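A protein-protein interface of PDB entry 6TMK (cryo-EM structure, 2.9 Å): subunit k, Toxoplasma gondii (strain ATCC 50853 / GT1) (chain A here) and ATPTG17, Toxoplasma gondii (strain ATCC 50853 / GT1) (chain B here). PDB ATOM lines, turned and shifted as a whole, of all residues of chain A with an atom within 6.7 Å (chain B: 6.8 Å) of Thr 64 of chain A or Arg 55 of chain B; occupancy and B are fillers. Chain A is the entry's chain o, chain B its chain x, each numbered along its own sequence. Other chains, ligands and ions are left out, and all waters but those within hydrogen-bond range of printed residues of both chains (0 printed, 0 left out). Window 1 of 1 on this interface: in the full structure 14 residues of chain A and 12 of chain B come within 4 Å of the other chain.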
ATOM      1  N   ARG A  59      14.578   0.363 -11.955  1.00  0.00           N
ATOM      2  CA  ARG A  59      14.494  -1.080 -12.128  1.00  0.00           C
ATOM      3  C   ARG A  59      14.171  -1.445 -13.568  1.00  0.00           C
ATOM      4  O   ARG A  59      14.752  -2.383 -14.119  1.00  0.00           O
ATOM      5  CB  ARG A  59      13.442  -1.657 -11.186  1.00  0.00           C
ATOM      6  CG  ARG A  59      13.317  -3.162 -11.231  1.00  0.00           C
ATOM      7  CD  ARG A  59      14.573  -3.830 -10.759  1.00  0.00           C
ATOM      8  NE  ARG A  59      14.454  -5.283 -10.783  1.00  0.00           N
ATOM      9  CZ  ARG A  59      14.806  -6.094  -9.792  1.00  0.00           C
ATOM     10  NH1 ARG A  59      14.652  -7.397  -9.935  1.00  0.00           N
ATOM     11  NH2 ARG A  59      15.308  -5.617  -8.665  1.00  0.00           N
ATOM     12  N   PHE A  60      13.240  -0.725 -14.189  1.00  0.00           N
ATOM     13  CA  PHE A  60      12.887  -0.995 -15.574  1.00  0.00           C
ATOM     14  C   PHE A  60      14.085  -0.788 -16.489  1.00  0.00           C
ATOM     15  O   PHE A  60      14.382  -1.627 -17.346  1.00  0.00           O
ATOM     16  CB  PHE A  60      11.726  -0.092 -15.980  1.00  0.00           C
ATOM     17  CG  PHE A  60      11.018  -0.535 -17.211  1.00  0.00           C
ATOM     18  CD1 PHE A  60      10.088  -1.548 -17.152  1.00  0.00           C
ATOM     19  CD2 PHE A  60      11.273   0.060 -18.425  1.00  0.00           C
ATOM     20  CE1 PHE A  60       9.432  -1.961 -18.278  1.00  0.00           C
ATOM     21  CE2 PHE A  60      10.616  -0.352 -19.555  1.00  0.00           C
ATOM     22  CZ  PHE A  60       9.695  -1.363 -19.479  1.00  0.00           C
ATOM     23  N   ARG A  61      14.788   0.330 -16.314  1.00  0.00           N
ATOM     24  CA  ARG A  61      15.957   0.620 -17.131  1.00  0.00           C
ATOM     25  C   ARG A  61      17.020  -0.456 -16.982  1.00  0.00           C
ATOM     26  O   ARG A  61      17.600  -0.907 -17.975  1.00  0.00           O
ATOM     27  CB  ARG A  61      16.505   1.987 -16.746  1.00  0.00           C
ATOM     28  CG  ARG A  61      17.686   2.454 -17.540  1.00  0.00           C
ATOM     29  CD  ARG A  61      18.128   3.799 -17.049  1.00  0.00           C
ATOM     30  NE  ARG A  61      18.605   3.727 -15.675  1.00  0.00           N
ATOM     31  CZ  ARG A  61      19.206   4.722 -15.036  1.00  0.00           C
ATOM     32  NH1 ARG A  61      19.406   5.879 -15.641  1.00  0.00           N
ATOM     33  NH2 ARG A  61      19.602   4.554 -13.787  1.00  0.00           N
ATOM     34  N   ALA A  62      17.293  -0.880 -15.752  1.00  0.00           N
ATOM     35  CA  ALA A  62      18.318  -1.892 -15.537  1.00  0.00           C
ATOM     36  C   ALA A  62      17.900  -3.236 -16.118  1.00  0.00           C
ATOM     37  O   ALA A  62      18.688  -3.902 -16.797  1.00  0.00           O
ATOM     38  CB  ALA A  62      18.610  -2.026 -14.048  1.00  0.00           C
ATOM     39  N   ASP A  63      16.669  -3.660 -15.843  1.00  0.00           N
ATOM     40  CA  ASP A  63      16.208  -4.977 -16.248  1.00  0.00           C
ATOM     41  C   ASP A  63      15.934  -5.065 -17.742  1.00  0.00           C
ATOM     42  O   ASP A  63      15.838  -6.175 -18.273  1.00  0.00           O
ATOM     43  CB  ASP A  63      14.952  -5.333 -15.462  1.00  0.00           C
ATOM     44  CG  ASP A  63      15.241  -5.648 -14.008  1.00  0.00           C
ATOM     45  OD1 ASP A  63      14.314  -6.088 -13.296  1.00  0.00           O
ATOM     46  OD2 ASP A  63      16.396  -5.462 -13.575  1.00  0.00           O
ATOM     47  N   THR A  64      15.790  -3.933 -18.425  1.00  0.00           N
ATOM     48  CA  THR A  64      15.398  -3.913 -19.827  1.00  0.00           C
ATOM     49  C   THR A  64      16.526  -3.420 -20.721  1.00  0.00           C
ATOM     50  O   THR A  64      16.914  -4.112 -21.664  1.00  0.00           O
ATOM     51  CB  THR A  64      14.153  -3.037 -20.013  1.00  0.00           C
ATOM     52  OG1 THR A  64      13.070  -3.563 -19.236  1.00  0.00           O
ATOM     53  CG2 THR A  64      13.749  -2.980 -21.460  1.00  0.00           C
ATOM     54  N   LYS A  65      17.054  -2.231 -20.464  1.00  0.00           N
ATOM     55  CA  LYS A  65      18.133  -1.720 -21.283  1.00  0.00           C
ATOM     56  C   LYS A  65      19.445  -2.401 -20.906  1.00  0.00           C
ATOM     57  O   LYS A  65      19.529  -3.164 -19.941  1.00  0.00           O
ATOM     58  CB  LYS A  65      18.248  -0.206 -21.144  1.00  0.00           C
ATOM     59  CG  LYS A  65      17.082   0.549 -21.730  1.00  0.00           C
ATOM     60  CD  LYS A  65      17.289   2.037 -21.653  1.00  0.00           C
ATOM     61  CE  LYS A  65      17.467   2.639 -23.031  1.00  0.00           C
ATOM     62  NZ  LYS A  65      17.933   4.053 -22.976  1.00  0.00           N
ATOM     63  N   LEU A  66      20.480  -2.118 -21.685  1.00  0.00           N
ATOM     64  CA  LEU A  66      21.794  -2.706 -21.486  1.00  0.00           C
ATOM     65  C   LEU A  66      22.833  -1.600 -21.525  1.00  0.00           C
ATOM     66  O   LEU A  66      22.815  -0.762 -22.429  1.00  0.00           O
ATOM     67  CB  LEU A  66      22.056  -3.783 -22.543  1.00  0.00           C
ATOM     68  CG  LEU A  66      22.371  -3.370 -23.970  1.00  0.00           C
ATOM     69  CD1 LEU A  66      22.802  -4.589 -24.709  1.00  0.00           C
ATOM     70  CD2 LEU A  66      21.189  -2.748 -24.651  1.00  0.00           C
ATOM     71  N   LEU A  98      22.277   2.409 -23.319  1.00  0.00           N
ATOM     72  CA  LEU A  98      22.072   2.665 -24.733  1.00  0.00           C
ATOM     73  C   LEU A  98      20.965   1.772 -25.267  1.00  0.00           C
ATOM     74  O   LEU A  98      20.524   0.821 -24.617  1.00  0.00           O
ATOM     75  CB  LEU A  98      23.353   2.424 -25.533  1.00  0.00           C
ATOM     76  CG  LEU A  98      24.613   3.157 -25.090  1.00  0.00           C
ATOM     77  CD1 LEU A  98      25.777   2.716 -25.930  1.00  0.00           C
ATOM     78  CD2 LEU A  98      24.429   4.646 -25.194  1.00  0.00           C
ATOM     79  N   ASP A 100      19.515  -0.701 -28.545  1.00  0.00           N
ATOM     80  CA  ASP A 100      20.106  -1.770 -29.337  1.00  0.00           C
ATOM     81  C   ASP A 100      20.533  -1.288 -30.717  1.00  0.00           C
ATOM     82  O   ASP A 100      21.436  -1.870 -31.323  1.00  0.00           O
ATOM     83  CB  ASP A 100      19.117  -2.921 -29.464  1.00  0.00           C
ATOM     84  CG  ASP A 100      18.795  -3.560 -28.130  1.00  0.00           C
ATOM     85  OD1 ASP A 100      19.453  -3.212 -27.128  1.00  0.00           O
ATOM     86  OD2 ASP A 100      17.879  -4.408 -28.083  1.00  0.00           O
ATOM     87  N   ALA A 137      26.051  -3.151 -29.671  1.00  0.00           N
ATOM     88  CA  ALA A 137      25.602  -4.370 -29.014  1.00  0.00           C
ATOM     89  C   ALA A 137      26.228  -5.600 -29.650  1.00  0.00           C
ATOM     90  O   ALA A 137      26.778  -6.463 -28.956  1.00  0.00           O
ATOM     91  CB  ALA A 137      24.080  -4.446 -29.062  1.00  0.00           C
ATOM     92  N   MET A 138      26.160  -5.696 -30.977  1.00  0.00           N
ATOM     93  CA  MET A 138      26.703  -6.862 -31.658  1.00  0.00           C
ATOM     94  C   MET A 138      28.221  -6.873 -31.608  1.00  0.00           C
ATOM     95  O   MET A 138      28.837  -7.940 -31.504  1.00  0.00           O
ATOM     96  CB  MET A 138      26.216  -6.886 -33.101  1.00  0.00           C
ATOM     97  CG  MET A 138      24.723  -6.728 -33.273  1.00  0.00           C
ATOM     98  SD  MET A 138      23.753  -7.606 -32.047  1.00  0.00           S
ATOM     99  CE  MET A 138      23.876  -9.255 -32.708  1.00  0.00           C
ATOM    100  N   ARG A 141      28.989  -8.211 -28.239  1.00  0.00           N
ATOM    101  CA  ARG A 141      28.691  -9.635 -28.268  1.00  0.00           C
ATOM    102  C   ARG A 141      29.815 -10.421 -28.924  1.00  0.00           C
ATOM    103  O   ARG A 141      30.166 -11.519 -28.476  1.00  0.00           O
ATOM    104  CB  ARG A 141      27.379  -9.857 -29.011  1.00  0.00           C
ATOM    105  CG  ARG A 141      26.803 -11.235 -28.907  1.00  0.00           C
ATOM    106  CD  ARG A 141      25.654 -11.373 -29.867  1.00  0.00           C
ATOM    107  NE  ARG A 141      24.750 -12.469 -29.526  1.00  0.00           N
ATOM    108  CZ  ARG A 141      24.827 -13.692 -30.036  1.00  0.00           C
ATOM    109  NH1 ARG A 141      25.768 -14.002 -30.914  1.00  0.00           N
ATOM    110  NH2 ARG A 141      23.956 -14.612 -29.667  1.00  0.00           N
ATOM    111  N   ALA B  26       6.019  -5.458 -14.580  1.00  0.00           N
ATOM    112  CA  ALA B  26       5.991  -4.664 -15.800  1.00  0.00           C
ATOM    113  C   ALA B  26       7.029  -5.154 -16.797  1.00  0.00           C
ATOM    114  O   ALA B  26       6.764  -5.219 -18.002  1.00  0.00           O
ATOM    115  CB  ALA B  26       6.231  -3.197 -15.462  1.00  0.00           C
ATOM    116  N   VAL B  27       8.222  -5.495 -16.312  1.00  0.00           N
ATOM    117  CA  VAL B  27       9.259  -6.036 -17.181  1.00  0.00           C
ATOM    118  C   VAL B  27       8.798  -7.341 -17.811  1.00  0.00           C
ATOM    119  O   VAL B  27       8.995  -7.577 -19.010  1.00  0.00           O
ATOM    120  CB  VAL B  27      10.559  -6.228 -16.383  1.00  0.00           C
ATOM    121  CG1 VAL B  27      11.537  -7.070 -17.158  1.00  0.00           C
ATOM    122  CG2 VAL B  27      11.172  -4.899 -16.038  1.00  0.00           C
ATOM    123  N   TRP B  30       6.249  -6.555 -20.525  1.00  0.00           N
ATOM    124  CA  TRP B  30       6.906  -6.005 -21.701  1.00  0.00           C
ATOM    125  C   TRP B  30       7.593  -7.103 -22.496  1.00  0.00           C
ATOM    126  O   TRP B  30       7.561  -7.103 -23.733  1.00  0.00           O
ATOM    127  CB  TRP B  30       7.911  -4.934 -21.286  1.00  0.00           C
ATOM    128  CG  TRP B  30       8.723  -4.423 -22.416  1.00  0.00           C
ATOM    129  CD1 TRP B  30      10.043  -4.657 -22.648  1.00  0.00           C
ATOM    130  CD2 TRP B  30       8.268  -3.592 -23.486  1.00  0.00           C
ATOM    131  NE1 TRP B  30      10.442  -4.022 -23.794  1.00  0.00           N
ATOM    132  CE2 TRP B  30       9.369  -3.358 -24.328  1.00  0.00           C
ATOM    133  CE3 TRP B  30       7.036  -3.020 -23.811  1.00  0.00           C
ATOM    134  CZ2 TRP B  30       9.276  -2.579 -25.477  1.00  0.00           C
ATOM    135  CZ3 TRP B  30       6.945  -2.247 -24.949  1.00  0.00           C
ATOM    136  CH2 TRP B  30       8.058  -2.032 -25.768  1.00  0.00           C
ATOM    137  N   ARG B  31       8.218  -8.052 -21.799  1.00  0.00           N
ATOM    138  CA  ARG B  31       8.868  -9.160 -22.485  1.00  0.00           C
ATOM    139  C   ARG B  31       7.861 -10.000 -23.251  1.00  0.00           C
ATOM    140  O   ARG B  31       8.110 -10.386 -24.401  1.00  0.00           O
ATOM    141  CB  ARG B  31       9.630 -10.013 -21.479  1.00  0.00           C
ATOM    142  CG  ARG B  31      10.908  -9.379 -21.012  1.00  0.00           C
ATOM    143  CD  ARG B  31      11.580 -10.204 -19.949  1.00  0.00           C
ATOM    144  NE  ARG B  31      12.773  -9.545 -19.431  1.00  0.00           N
ATOM    145  CZ  ARG B  31      13.275  -9.746 -18.220  1.00  0.00           C
ATOM    146  NH1 ARG B  31      12.700 -10.597 -17.383  1.00  0.00           N
ATOM    147  NH2 ARG B  31      14.364  -9.097 -17.853  1.00  0.00           N
ATOM    148  N   ASN B  34       6.841  -8.079 -26.391  1.00  0.00           N
ATOM    149  CA  ASN B  34       7.884  -8.115 -27.408  1.00  0.00           C
ATOM    150  C   ASN B  34       7.941  -9.478 -28.087  1.00  0.00           C
ATOM    151  O   ASN B  34       8.104  -9.565 -29.310  1.00  0.00           O
ATOM    152  CB  ASN B  34       9.228  -7.762 -26.783  1.00  0.00           C
ATOM    153  CG  ASN B  34       9.356  -6.286 -26.479  1.00  0.00           C
ATOM    154  OD1 ASN B  34       8.359  -5.574 -26.375  1.00  0.00           O
ATOM    155  ND2 ASN B  34      10.588  -5.816 -26.341  1.00  0.00           N
ATOM    156  N   TYR B  51      15.863 -14.775 -34.924  1.00  0.00           N
ATOM    157  CA  TYR B  51      16.099 -15.566 -33.727  1.00  0.00           C
ATOM    158  C   TYR B  51      15.184 -15.065 -32.616  1.00  0.00           C
ATOM    159  O   TYR B  51      15.300 -13.903 -32.214  1.00  0.00           O
ATOM    160  CB  TYR B  51      17.547 -15.458 -33.288  1.00  0.00           C
ATOM    161  CG  TYR B  51      18.561 -15.997 -34.263  1.00  0.00           C
ATOM    162  CD1 TYR B  51      18.583 -17.334 -34.601  1.00  0.00           C
ATOM    163  CD2 TYR B  51      19.510 -15.168 -34.831  1.00  0.00           C
ATOM    164  CE1 TYR B  51      19.512 -17.828 -35.483  1.00  0.00           C
ATOM    165  CE2 TYR B  51      20.440 -15.654 -35.711  1.00  0.00           C
ATOM    166  CZ  TYR B  51      20.438 -16.986 -36.035  1.00  0.00           C
ATOM    167  OH  TYR B  51      21.364 -17.480 -36.917  1.00  0.00           O
ATOM    168  N   PRO B  52      14.273 -15.889 -32.092  1.00  0.00           N
ATOM    169  CA  PRO B  52      13.267 -15.363 -31.161  1.00  0.00           C
ATOM    170  C   PRO B  52      13.844 -14.918 -29.829  1.00  0.00           C
ATOM    171  O   PRO B  52      13.570 -13.806 -29.369  1.00  0.00           O
ATOM    172  CB  PRO B  52      12.306 -16.545 -30.974  1.00  0.00           C
ATOM    173  CG  PRO B  52      12.737 -17.591 -31.916  1.00  0.00           C
ATOM    174  CD  PRO B  52      14.154 -17.345 -32.241  1.00  0.00           C
ATOM    175  N   SER B  53      14.640 -15.776 -29.201  1.00  0.00           N
ATOM    176  CA  SER B  53      15.143 -15.537 -27.859  1.00  0.00           C
ATOM    177  C   SER B  53      16.444 -14.753 -27.859  1.00  0.00           C
ATOM    178  O   SER B  53      17.183 -14.795 -26.870  1.00  0.00           O
ATOM    179  CB  SER B  53      15.331 -16.858 -27.115  1.00  0.00           C
ATOM    180  OG  SER B  53      14.108 -17.554 -26.974  1.00  0.00           O
ATOM    181  N   ASN B  54      16.736 -14.039 -28.937  1.00  0.00           N
ATOM    182  CA  ASN B  54      17.929 -13.219 -29.029  1.00  0.00           C
ATOM    183  C   ASN B  54      17.591 -11.753 -28.795  1.00  0.00           C
ATOM    184  O   ASN B  54      16.467 -11.305 -29.035  1.00  0.00           O
ATOM    185  CB  ASN B  54      18.581 -13.391 -30.398  1.00  0.00           C
ATOM    186  CG  ASN B  54      19.207 -14.754 -30.579  1.00  0.00           C
ATOM    187  OD1 ASN B  54      18.637 -15.770 -30.185  1.00  0.00           O
ATOM    188  ND2 ASN B  54      20.380 -14.787 -31.187  1.00  0.00           N
ATOM    189  N   ARG B  55      18.593 -11.009 -28.330  1.00  0.00           N
ATOM    190  CA  ARG B  55      18.389  -9.620 -27.936  1.00  0.00           C
ATOM    191  C   ARG B  55      17.997  -8.752 -29.123  1.00  0.00           C
ATOM    192  O   ARG B  55      17.007  -8.013 -29.067  1.00  0.00           O
ATOM    193  CB  ARG B  55      19.668  -9.099 -27.279  1.00  0.00           C
ATOM    194  CG  ARG B  55      19.626  -7.678 -26.766  1.00  0.00           C
ATOM    195  CD  ARG B  55      18.823  -7.553 -25.503  1.00  0.00           C
ATOM    196  NE  ARG B  55      18.418  -6.173 -25.268  1.00  0.00           N
ATOM    197  CZ  ARG B  55      17.929  -5.729 -24.117  1.00  0.00           C
ATOM    198  NH1 ARG B  55      17.780  -6.555 -23.096  1.00  0.00           N
ATOM    199  NH2 ARG B  55      17.587  -4.458 -23.991  1.00  0.00           N
ATOM    200  N   TYR B  56      18.755  -8.835 -30.213  1.00  0.00           N
ATOM    201  CA  TYR B  56      18.605  -7.921 -31.332  1.00  0.00           C
ATOM    202  C   TYR B  56      18.789  -8.691 -32.629  1.00  0.00           C
ATOM    203  O   TYR B  56      19.660  -9.559 -32.723  1.00  0.00           O
ATOM    204  CB  TYR B  56      19.626  -6.779 -31.235  1.00  0.00           C
ATOM    205  CG  TYR B  56      19.465  -5.675 -32.251  1.00  0.00           C
ATOM    206  CD1 TYR B  56      18.235  -5.084 -32.480  1.00  0.00           C
ATOM    207  CD2 TYR B  56      20.551  -5.214 -32.971  1.00  0.00           C
ATOM    208  CE1 TYR B  56      18.093  -4.076 -33.403  1.00  0.00           C
ATOM    209  CE2 TYR B  56      20.419  -4.207 -33.892  1.00  0.00           C
ATOM    210  CZ  TYR B  56      19.188  -3.642 -34.109  1.00  0.00           C
ATOM    211  OH  TYR B  56      19.058  -2.633 -35.032  1.00  0.00           O
ATOM    212  N   ASN B  57      17.958  -8.376 -33.622  1.00  0.00           N
ATOM    213  CA  ASN B  57      17.969  -9.048 -34.919  1.00  0.00           C
ATOM    214  C   ASN B  57      18.077  -7.993 -36.009  1.00  0.00           C
ATOM    215  O   ASN B  57      17.059  -7.518 -36.528  1.00  0.00           O
ATOM    216  CB  ASN B  57      16.718  -9.897 -35.112  1.00  0.00           C
ATOM    217  CG  ASN B  57      16.856 -11.280 -34.531  1.00  0.00           C
ATOM    218  OD1 ASN B  57      17.569 -12.126 -35.065  1.00  0.00           O
ATOM    219  ND2 ASN B  57      16.170 -11.521 -33.431  1.00  0.00           N
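Hydrophobic or aromatic side chains of chain B within 4 Å of the printed part of chain A: Val 27 and Tyr 56.
Along chain B the printed residues that touch a printed residue of chain A span positions 27 to 56.
Printed residues of chain A that touch a printed residue of chain B: Phe 60, Asp 63, Thr 64, Lys 65, Asp 100 and Arg 141.
Among the printed residues, 9 pairs touch across the chains.
Among the printed residues, Asp or Glu carboxylates within 4 Å of a Lys or Arg side-chain nitrogen of the other chain: Asp 100 of chain A with Arg 55 of chain B (3.4 Å).
Printed residues of chain B within 4 Å of Thr 64 of chain A: Val 27 and Arg 55.
Of chain A, only Thr 64 (2.4 Å), Lys 65 (3.9 Å) and Asp 100 (3.4 Å) come within 4 Å of Arg 55 of chain B.
Printed residues of chain B within 4 Å of Asp 100 of chain A: Arg 55 (3.4 Å) and Tyr 56 (3.6 Å).
Printed residues of chain B within 4 Å of Lys 65 of chain A: Arg 55 (3.9 Å).
Of the printed residues of chain A, Val 27 of chain B touches Phe 60, Asp 63 and Thr 64.
The nearest residue of chain A that does not touch Arg 55 of chain B is Leu 66 of chain A (4.04 Å).
The nearest printed residue of chain B that does not touch Lys 65 of chain A is Trp 30 of chain B (7.6 Å).
The backbone carbonyl oxygen of Phe 60 of chain A lies within hydrogen-bond range of the side-chain hydroxyl of Thr 64 of chain A.
The guanidinium group (NE) of Arg 59 of chain A is in salt-bridge range of the side-chain carboxylate (OD1) of Asp 63 of chain A (2.6 Å).
Among the printed residues, pairs that only touch across the chains: Phe 60 of chain A with Val 27 of chain B (3.7 Å), Asp 63 of chain A with Val 27 of chain B (3.8 Å), Thr 64 of chain A with Val 27 of chain B (3.95 Å), Lys 65 of chain A with Arg 55 of chain B (3.9 Å), Asp 100 of chain A with Tyr 56 of chain B (3.6 Å) and Arg 141 of chain A with Asn 54 of chain B (3.9 Å).
NH2 of Arg 31 of chain B lies within hydrogen-bond range of O of Asp 63 of chain A (3.3 Å).
NE of Arg 55 of chain B is in salt-bridge range of OD2 of Asp 100 of chain A (3.4 Å).
The guanidinium group (NH2) of Arg 55 of chain B sits at hydrogen-bond distance from the backbone carbonyl oxygen (O) of Thr 64 of chain A (2.4 Å).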
